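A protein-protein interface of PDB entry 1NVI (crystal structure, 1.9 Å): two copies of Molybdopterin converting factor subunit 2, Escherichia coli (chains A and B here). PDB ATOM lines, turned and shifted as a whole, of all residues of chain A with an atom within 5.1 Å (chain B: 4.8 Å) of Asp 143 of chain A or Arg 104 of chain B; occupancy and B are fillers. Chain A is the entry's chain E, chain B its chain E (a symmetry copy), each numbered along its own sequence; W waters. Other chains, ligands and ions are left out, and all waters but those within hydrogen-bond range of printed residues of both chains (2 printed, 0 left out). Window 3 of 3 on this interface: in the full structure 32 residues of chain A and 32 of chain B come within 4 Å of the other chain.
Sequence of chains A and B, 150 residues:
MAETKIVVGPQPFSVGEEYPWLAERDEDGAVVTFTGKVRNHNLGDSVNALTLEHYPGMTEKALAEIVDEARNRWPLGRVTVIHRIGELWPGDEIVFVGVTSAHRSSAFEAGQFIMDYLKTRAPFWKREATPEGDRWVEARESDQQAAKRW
The guanidinium group (NH2) of Arg 104 of chain B is in salt-bridge range of the side-chain carboxylate (OD1) of Asp 143 of chain A (2.9 Å). NH2 of Arg 104 of chain B lies within salt-bridge range of OD1 of Asp 116 of chain A (2.8 Å).
O of Asp 116 of chain A is in hydrogen-bond range of OG1 of Thr 120 of chain A, 3.2 Å away.
Phe 34 of chain A touches Ala 30 of chain B (CE1 to CB, 3.6 Å). CB of Arg 104 of chain B touches CE1 of Phe 34 of chain A, at 3.4 Å. CB of Phe 34 of chain A touches CZ of Phe 108 of chain B (3.6 Å). Gln 112 of chain A touches Ser 105 of chain B. CZ of Phe 108 of chain B touches N of Gln 112 of chain A, at 3.7 Å. Lys 119 of chain A touches Arg 104 of chain B (CD to NH1, 3.2 Å). CE1 of His 103 of chain B touches NH2 of Arg 140 of chain A, 3.98 Å away. NH2 of Arg 104 of chain B touches CB of Ala 146 of chain A, 3.97 Å away.
Of the printed residues of chain B, Gln 112 of chain A touches Ser 105 and Phe 108. Met 115 of chain A touches none of the printed residues of chain B. Of the printed residues of chain B, Asp 116 of chain A touches Arg 104. Printed residues of chain B within 4 Å of Ala 146 of chain A: Arg 104 (3.97 Å). Of chain A, only Phe 34 (3.4 Å), Asp 116 (2.8 Å), Lys 119 (3.2 Å), Asp 143 (2.9 Å) and Ala 146 (3.97 Å) come within 4 Å of Arg 104 of chain B. The nearest printed residue of chain B that does not touch Ala 146 of chain A is Ser 105 of chain B (6.9 Å).
Hydrophobic or aromatic side chains of chain B within 4 Å of the printed part of chain A: Ala 30, His 103 and Phe 108. Of the 14 printed residues of chain A, 7 touch a printed residue of chain B. Among the printed residues, Asp or Glu carboxylates within 4 Å of a Lys or Arg side-chain nitrogen of the other chain: Asp 116 of chain A with Arg 104 of chain B (2.8 Å) and Asp 143 of chain A with Arg 104 of chain B (2.9 Å).
No position is printed for both chains. Of the 10 pairs that touch across the chains among the printed residues, none has its exchanged pair printed and touching as well.
Water W2 lies within hydrogen-bond range of the backbone carbonyl oxygen of Asp 116 of chain A (2.7 Å), the backbone carbonyl oxygen of Asp 143 of chain A (2.7 Å) and the guanidinium group of Arg 104 of chain B (2.9 Å). Water W1 lies within hydrogen-bond range of the guanidinium group of Arg 104 of chain B (3.0 Å), the backbone carbonyl oxygen of Gln 112 of chain A (3.1 Å) and the side-chain carboxylate of Asp 116 of chain A (3.2 Å).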
ATOM      1  N   PHE A  34     -18.430   5.524   7.677  1.00  0.00           N
ATOM      2  CA  PHE A  34     -17.040   5.743   7.368  1.00  0.00           C
ATOM      3  C   PHE A  34     -16.678   7.190   7.715  1.00  0.00           C
ATOM      4  O   PHE A  34     -17.370   8.127   7.305  1.00  0.00           O
ATOM      5  CB  PHE A  34     -16.712   5.489   5.882  1.00  0.00           C
ATOM      6  CG  PHE A  34     -15.289   5.874   5.518  1.00  0.00           C
ATOM      7  CD1 PHE A  34     -14.254   4.988   5.693  1.00  0.00           C
ATOM      8  CD2 PHE A  34     -14.999   7.155   5.041  1.00  0.00           C
ATOM      9  CE1 PHE A  34     -12.942   5.377   5.412  1.00  0.00           C
ATOM     10  CE2 PHE A  34     -13.717   7.533   4.742  1.00  0.00           C
ATOM     11  CZ  PHE A  34     -12.689   6.661   4.934  1.00  0.00           C
ATOM     12  N   GLN A 112     -18.824   1.850   0.734  1.00  0.00           N
ATOM     13  CA  GLN A 112     -17.516   1.874   0.062  1.00  0.00           C
ATOM     14  C   GLN A 112     -17.645   2.444  -1.358  1.00  0.00           C
ATOM     15  O   GLN A 112     -16.789   3.217  -1.817  1.00  0.00           O
ATOM     16  CB  GLN A 112     -16.870   0.472   0.055  1.00  0.00           C
ATOM     17  CG  GLN A 112     -15.441   0.453  -0.501  1.00  0.00           C
ATOM     18  CD  GLN A 112     -14.656  -0.839  -0.223  1.00  0.00           C
ATOM     19  OE1 GLN A 112     -13.418  -0.829  -0.286  1.00  0.00           O
ATOM     20  NE2 GLN A 112     -15.358  -1.932   0.071  1.00  0.00           N
ATOM     21  N   MET A 115     -17.790   6.251  -1.225  1.00  0.00           N
ATOM     22  CA  MET A 115     -16.475   6.837  -0.997  1.00  0.00           C
ATOM     23  C   MET A 115     -15.601   6.749  -2.251  1.00  0.00           C
ATOM     24  O   MET A 115     -14.852   7.684  -2.547  1.00  0.00           O
ATOM     25  CB  MET A 115     -15.757   6.171   0.194  1.00  0.00           C
ATOM     26  CG  MET A 115     -16.098   6.783   1.567  1.00  0.00           C
ATOM     27  SD  MET A 115     -15.798   8.583   1.669  1.00  0.00           S
ATOM     28  CE  MET A 115     -14.075   8.607   1.370  1.00  0.00           C
ATOM     29  N   ASP A 116     -15.675   5.627  -2.961  1.00  0.00           N
ATOM     30  CA  ASP A 116     -14.851   5.417  -4.154  1.00  0.00           C
ATOM     31  C   ASP A 116     -15.218   6.428  -5.224  1.00  0.00           C
ATOM     32  O   ASP A 116     -14.350   7.007  -5.882  1.00  0.00           O
ATOM     33  CB  ASP A 116     -15.039   4.000  -4.717  1.00  0.00           C
ATOM     34  CG  ASP A 116     -14.370   2.941  -3.865  1.00  0.00           C
ATOM     35  OD1 ASP A 116     -13.504   3.279  -3.034  1.00  0.00           O
ATOM     36  OD2 ASP A 116     -14.674   1.737  -3.932  1.00  0.00           O
ATOM     37  N   LYS A 119     -14.275  10.059  -4.236  1.00  0.00           N
ATOM     38  CA  LYS A 119     -12.849  10.277  -4.458  1.00  0.00           C
ATOM     39  C   LYS A 119     -12.483  10.499  -5.913  1.00  0.00           C
ATOM     40  O   LYS A 119     -11.389  10.979  -6.191  1.00  0.00           O
ATOM     41  CB  LYS A 119     -12.024   9.106  -3.901  1.00  0.00           C
ATOM     42  CG  LYS A 119     -11.993   9.096  -2.374  1.00  0.00           C
ATOM     43  CD  LYS A 119     -10.709   8.523  -1.828  1.00  0.00           C
ATOM     44  CE  LYS A 119      -9.648   9.572  -1.678  1.00  0.00           C
ATOM     45  NZ  LYS A 119      -9.696  10.141  -0.335  1.00  0.00           N
ATOM     46  N   THR A 120     -13.366  10.133  -6.840  1.00  0.00           N
ATOM     47  CA  THR A 120     -13.087  10.308  -8.272  1.00  0.00           C
ATOM     48  C   THR A 120     -14.004  11.275  -8.995  1.00  0.00           C
ATOM     49  O   THR A 120     -13.691  11.703 -10.110  1.00  0.00           O
ATOM     50  CB  THR A 120     -13.151   8.950  -9.009  1.00  0.00           C
ATOM     51  OG1 THR A 120     -14.416   8.315  -8.764  1.00  0.00           O
ATOM     52  CG2 THR A 120     -12.090   7.999  -8.469  1.00  0.00           C
ATOM     53  N   ARG A 140      -4.632   9.538  -7.177  1.00  0.00           N
ATOM     54  CA  ARG A 140      -4.117   8.182  -7.317  1.00  0.00           C
ATOM     55  C   ARG A 140      -4.937   7.369  -8.319  1.00  0.00           C
ATOM     56  O   ARG A 140      -6.176   7.362  -8.276  1.00  0.00           O
ATOM     57  CB  ARG A 140      -4.149   7.487  -5.960  1.00  0.00           C
ATOM     58  CG  ARG A 140      -3.258   8.160  -4.915  1.00  0.00           C
ATOM     59  CD  ARG A 140      -2.962   7.288  -3.700  1.00  0.00           C
ATOM     60  NE  ARG A 140      -3.565   7.807  -2.465  1.00  0.00           N
ATOM     61  CZ  ARG A 140      -2.949   7.891  -1.275  1.00  0.00           C
ATOM     62  NH1 ARG A 140      -1.681   7.496  -1.116  1.00  0.00           N
ATOM     63  NH2 ARG A 140      -3.615   8.379  -0.228  1.00  0.00           N
ATOM     64  N   GLU A 141      -4.228   6.673  -9.206  1.00  0.00           N
ATOM     65  CA  GLU A 141      -4.848   5.755 -10.159  1.00  0.00           C
ATOM     66  C   GLU A 141      -5.598   4.637  -9.429  1.00  0.00           C
ATOM     67  O   GLU A 141      -6.609   4.167  -9.925  1.00  0.00           O
ATOM     68  CB  GLU A 141      -3.799   5.161 -11.101  1.00  0.00           C
ATOM     69  CG  GLU A 141      -4.344   4.202 -12.161  1.00  0.00           C
ATOM     70  CD  GLU A 141      -5.317   4.859 -13.132  1.00  0.00           C
ATOM     71  OE1 GLU A 141      -5.338   6.107 -13.243  1.00  0.00           O
ATOM     72  OE2 GLU A 141      -6.067   4.119 -13.794  1.00  0.00           O
ATOM     73  N   SER A 142      -5.101   4.234  -8.257  1.00  0.00           N
ATOM     74  CA  SER A 142      -5.742   3.197  -7.453  1.00  0.00           C
ATOM     75  C   SER A 142      -7.171   3.567  -7.081  1.00  0.00           C
ATOM     76  O   SER A 142      -8.013   2.687  -6.974  1.00  0.00           O
ATOM     77  CB  SER A 142      -4.926   2.877  -6.184  1.00  0.00           C
ATOM     78  OG  SER A 142      -4.854   3.992  -5.314  1.00  0.00           O
ATOM     79  N   ASP A 143      -7.450   4.858  -6.879  1.00  0.00           N
ATOM     80  CA  ASP A 143      -8.829   5.301  -6.682  1.00  0.00           C
ATOM     81  C   ASP A 143      -9.693   5.185  -7.944  1.00  0.00           C
ATOM     82  O   ASP A 143     -10.874   4.878  -7.825  1.00  0.00           O
ATOM     83  CB  ASP A 143      -8.903   6.721  -6.135  1.00  0.00           C
ATOM     84  CG  ASP A 143      -8.362   6.824  -4.738  1.00  0.00           C
ATOM     85  OD1 ASP A 143      -8.635   5.920  -3.915  1.00  0.00           O
ATOM     86  OD2 ASP A 143      -7.655   7.775  -4.376  1.00  0.00           O
ATOM     87  N   GLN A 144      -9.119   5.429  -9.128  1.00  0.00           N
ATOM     88  CA  GLN A 144      -9.834   5.166 -10.387  1.00  0.00           C
ATOM     89  C   GLN A 144     -10.207   3.685 -10.497  1.00  0.00           C
ATOM     90  O   GLN A 144     -11.318   3.366 -10.899  1.00  0.00           O
ATOM     91  CB  GLN A 144      -9.028   5.596 -11.620  1.00  0.00           C
ATOM     92  CG  GLN A 144      -8.720   7.109 -11.705  1.00  0.00           C
ATOM     93  CD  GLN A 144      -9.963   7.964 -11.911  1.00  0.00           C
ATOM     94  OE1 GLN A 144     -10.916   7.531 -12.555  1.00  0.00           O
ATOM     95  NE2 GLN A 144      -9.952   9.180 -11.372  1.00  0.00           N
ATOM     96  N   GLN A 145      -9.285   2.794 -10.129  1.00  0.00           N
ATOM     97  CA  GLN A 145      -9.541   1.344 -10.140  1.00  0.00           C
ATOM     98  C   GLN A 145     -10.638   0.953  -9.146  1.00  0.00           C
ATOM     99  O   GLN A 145     -11.537   0.192  -9.481  1.00  0.00           O
ATOM    100  CB  GLN A 145      -8.254   0.567  -9.839  1.00  0.00           C
ATOM    101  CG  GLN A 145      -7.246   0.615 -11.008  1.00  0.00           C
ATOM    102  CD  GLN A 145      -5.824   0.259 -10.618  1.00  0.00           C
ATOM    103  OE1 GLN A 145      -4.925   0.307 -11.459  1.00  0.00           O
ATOM    104  NE2 GLN A 145      -5.614  -0.099  -9.360  1.00  0.00           N
ATOM    105  N   ALA A 146     -10.565   1.504  -7.943  1.00  0.00           N
ATOM    106  CA  ALA A 146     -11.573   1.271  -6.915  1.00  0.00           C
ATOM    107  C   ALA A 146     -12.971   1.697  -7.371  1.00  0.00           C
ATOM    108  O   ALA A 146     -13.958   1.052  -7.039  1.00  0.00           O
ATOM    109  CB  ALA A 146     -11.190   1.988  -5.638  1.00  0.00           C
ATOM    110  N   ALA A 147     -13.067   2.771  -8.145  1.00  0.00           N
ATOM    111  CA  ALA A 147     -14.376   3.264  -8.556  1.00  0.00           C
ATOM    112  C   ALA A 147     -14.969   2.449  -9.703  1.00  0.00           C
ATOM    113  O   ALA A 147     -16.172   2.135  -9.705  1.00  0.00           O
ATOM    114  CB  ALA A 147     -14.291   4.748  -8.938  1.00  0.00           C
ATOM    115  N   ALA B  30      -8.662   6.313   8.556  1.00  0.00           N
ATOM    116  CA  ALA B  30      -9.972   5.745   8.193  1.00  0.00           C
ATOM    117  C   ALA B  30     -10.614   5.061   9.387  1.00  0.00           C
ATOM    118  O   ALA B  30      -9.957   4.276  10.058  1.00  0.00           O
ATOM    119  CB  ALA B  30      -9.819   4.745   7.049  1.00  0.00           C
ATOM    120  N   ALA B 102      -4.917   2.976   8.215  1.00  0.00           N
ATOM    121  CA  ALA B 102      -4.358   4.129   7.552  1.00  0.00           C
ATOM    122  C   ALA B 102      -5.239   4.547   6.361  1.00  0.00           C
ATOM    123  O   ALA B 102      -5.413   5.742   6.110  1.00  0.00           O
ATOM    124  CB  ALA B 102      -2.922   3.839   7.111  1.00  0.00           C
ATOM    125  N   HIS B 103      -5.817   3.560   5.672  1.00  0.00           N
ATOM    126  CA  HIS B 103      -6.564   3.775   4.430  1.00  0.00           C
ATOM    127  C   HIS B 103      -7.902   3.056   4.455  1.00  0.00           C
ATOM    128  O   HIS B 103      -8.081   2.095   5.206  1.00  0.00           O
ATOM    129  CB  HIS B 103      -5.745   3.286   3.227  1.00  0.00           C
ATOM    130  CG  HIS B 103      -4.446   4.004   3.057  1.00  0.00           C
ATOM    131  ND1 HIS B 103      -4.378   5.348   2.759  1.00  0.00           N
ATOM    132  CD2 HIS B 103      -3.166   3.572   3.162  1.00  0.00           C
ATOM    133  CE1 HIS B 103      -3.107   5.715   2.691  1.00  0.00           C
ATOM    134  NE2 HIS B 103      -2.353   4.654   2.927  1.00  0.00           N
ATOM    135  N   ARG B 104      -8.827   3.497   3.600  1.00  0.00           N
ATOM    136  CA  ARG B 104     -10.228   3.095   3.718  1.00  0.00           C
ATOM    137  C   ARG B 104     -10.493   1.634   3.338  1.00  0.00           C
ATOM    138  O   ARG B 104     -11.339   0.995   3.956  1.00  0.00           O
ATOM    139  CB  ARG B 104     -11.156   4.024   2.918  1.00  0.00           C
ATOM    140  CG  ARG B 104     -11.071   3.931   1.411  1.00  0.00           C
ATOM    141  CD  ARG B 104     -11.807   5.053   0.713  1.00  0.00           C
ATOM    142  NE  ARG B 104     -11.891   4.843  -0.723  1.00  0.00           N
ATOM    143  CZ  ARG B 104     -10.928   5.092  -1.594  1.00  0.00           C
ATOM    144  NH1 ARG B 104      -9.754   5.588  -1.195  1.00  0.00           N
ATOM    145  NH2 ARG B 104     -11.135   4.840  -2.882  1.00  0.00           N
ATOM    146  N   SER B 105      -9.791   1.096   2.343  1.00  0.00           N
ATOM    147  CA  SER B 105     -10.146  -0.251   1.883  1.00  0.00           C
ATOM    148  C   SER B 105      -9.906  -1.315   2.987  1.00  0.00           C
ATOM    149  O   SER B 105     -10.711  -2.234   3.157  1.00  0.00           O
ATOM    150  CB  SER B 105      -9.480  -0.611   0.552  1.00  0.00           C
ATOM    151  OG  SER B 105      -8.102  -0.829   0.691  1.00  0.00           O
ATOM    152  N   SER B 106      -8.838  -1.160   3.759  1.00  0.00           N
ATOM    153  CA  SER B 106      -8.558  -2.084   4.854  1.00  0.00           C
ATOM    154  C   SER B 106      -9.621  -2.005   5.954  1.00  0.00           C
ATOM    155  O   SER B 106     -10.038  -3.034   6.498  1.00  0.00           O
ATOM    156  CB  SER B 106      -7.167  -1.815   5.428  1.00  0.00           C
ATOM    157  OG  SER B 106      -6.199  -2.308   4.539  1.00  0.00           O
ATOM    158  N   ALA B 107     -10.075  -0.803   6.275  1.00  0.00           N
ATOM    159  CA  ALA B 107     -11.095  -0.643   7.304  1.00  0.00           C
ATOM    160  C   ALA B 107     -12.452  -1.256   6.871  1.00  0.00           C
ATOM    161  O   ALA B 107     -13.098  -1.952   7.655  1.00  0.00           O
ATOM    162  CB  ALA B 107     -11.237   0.815   7.684  1.00  0.00           C
ATOM    163  N   PHE B 108     -12.847  -1.038   5.621  1.00  0.00           N
ATOM    164  CA  PHE B 108     -14.109  -1.574   5.103  1.00  0.00           C
ATOM    165  C   PHE B 108     -14.063  -3.101   5.035  1.00  0.00           C
ATOM    166  O   PHE B 108     -15.040  -3.794   5.383  1.00  0.00           O
ATOM    167  CB  PHE B 108     -14.403  -1.037   3.700  1.00  0.00           C
ATOM    168  CG  PHE B 108     -15.161   0.275   3.672  1.00  0.00           C
ATOM    169  CD1 PHE B 108     -14.579   1.413   3.139  1.00  0.00           C
ATOM    170  CD2 PHE B 108     -16.451   0.368   4.168  1.00  0.00           C
ATOM    171  CE1 PHE B 108     -15.265   2.620   3.108  1.00  0.00           C
ATOM    172  CE2 PHE B 108     -17.149   1.552   4.119  1.00  0.00           C
ATOM    173  CZ  PHE B 108     -16.564   2.684   3.592  1.00  0.00           C
HETATM  174  O   HOH W   1     -14.326   3.249   0.102  1.00  0.00           O
HETATM  175  O   HOH W   2     -12.063   5.669  -5.548  1.00  0.00           O
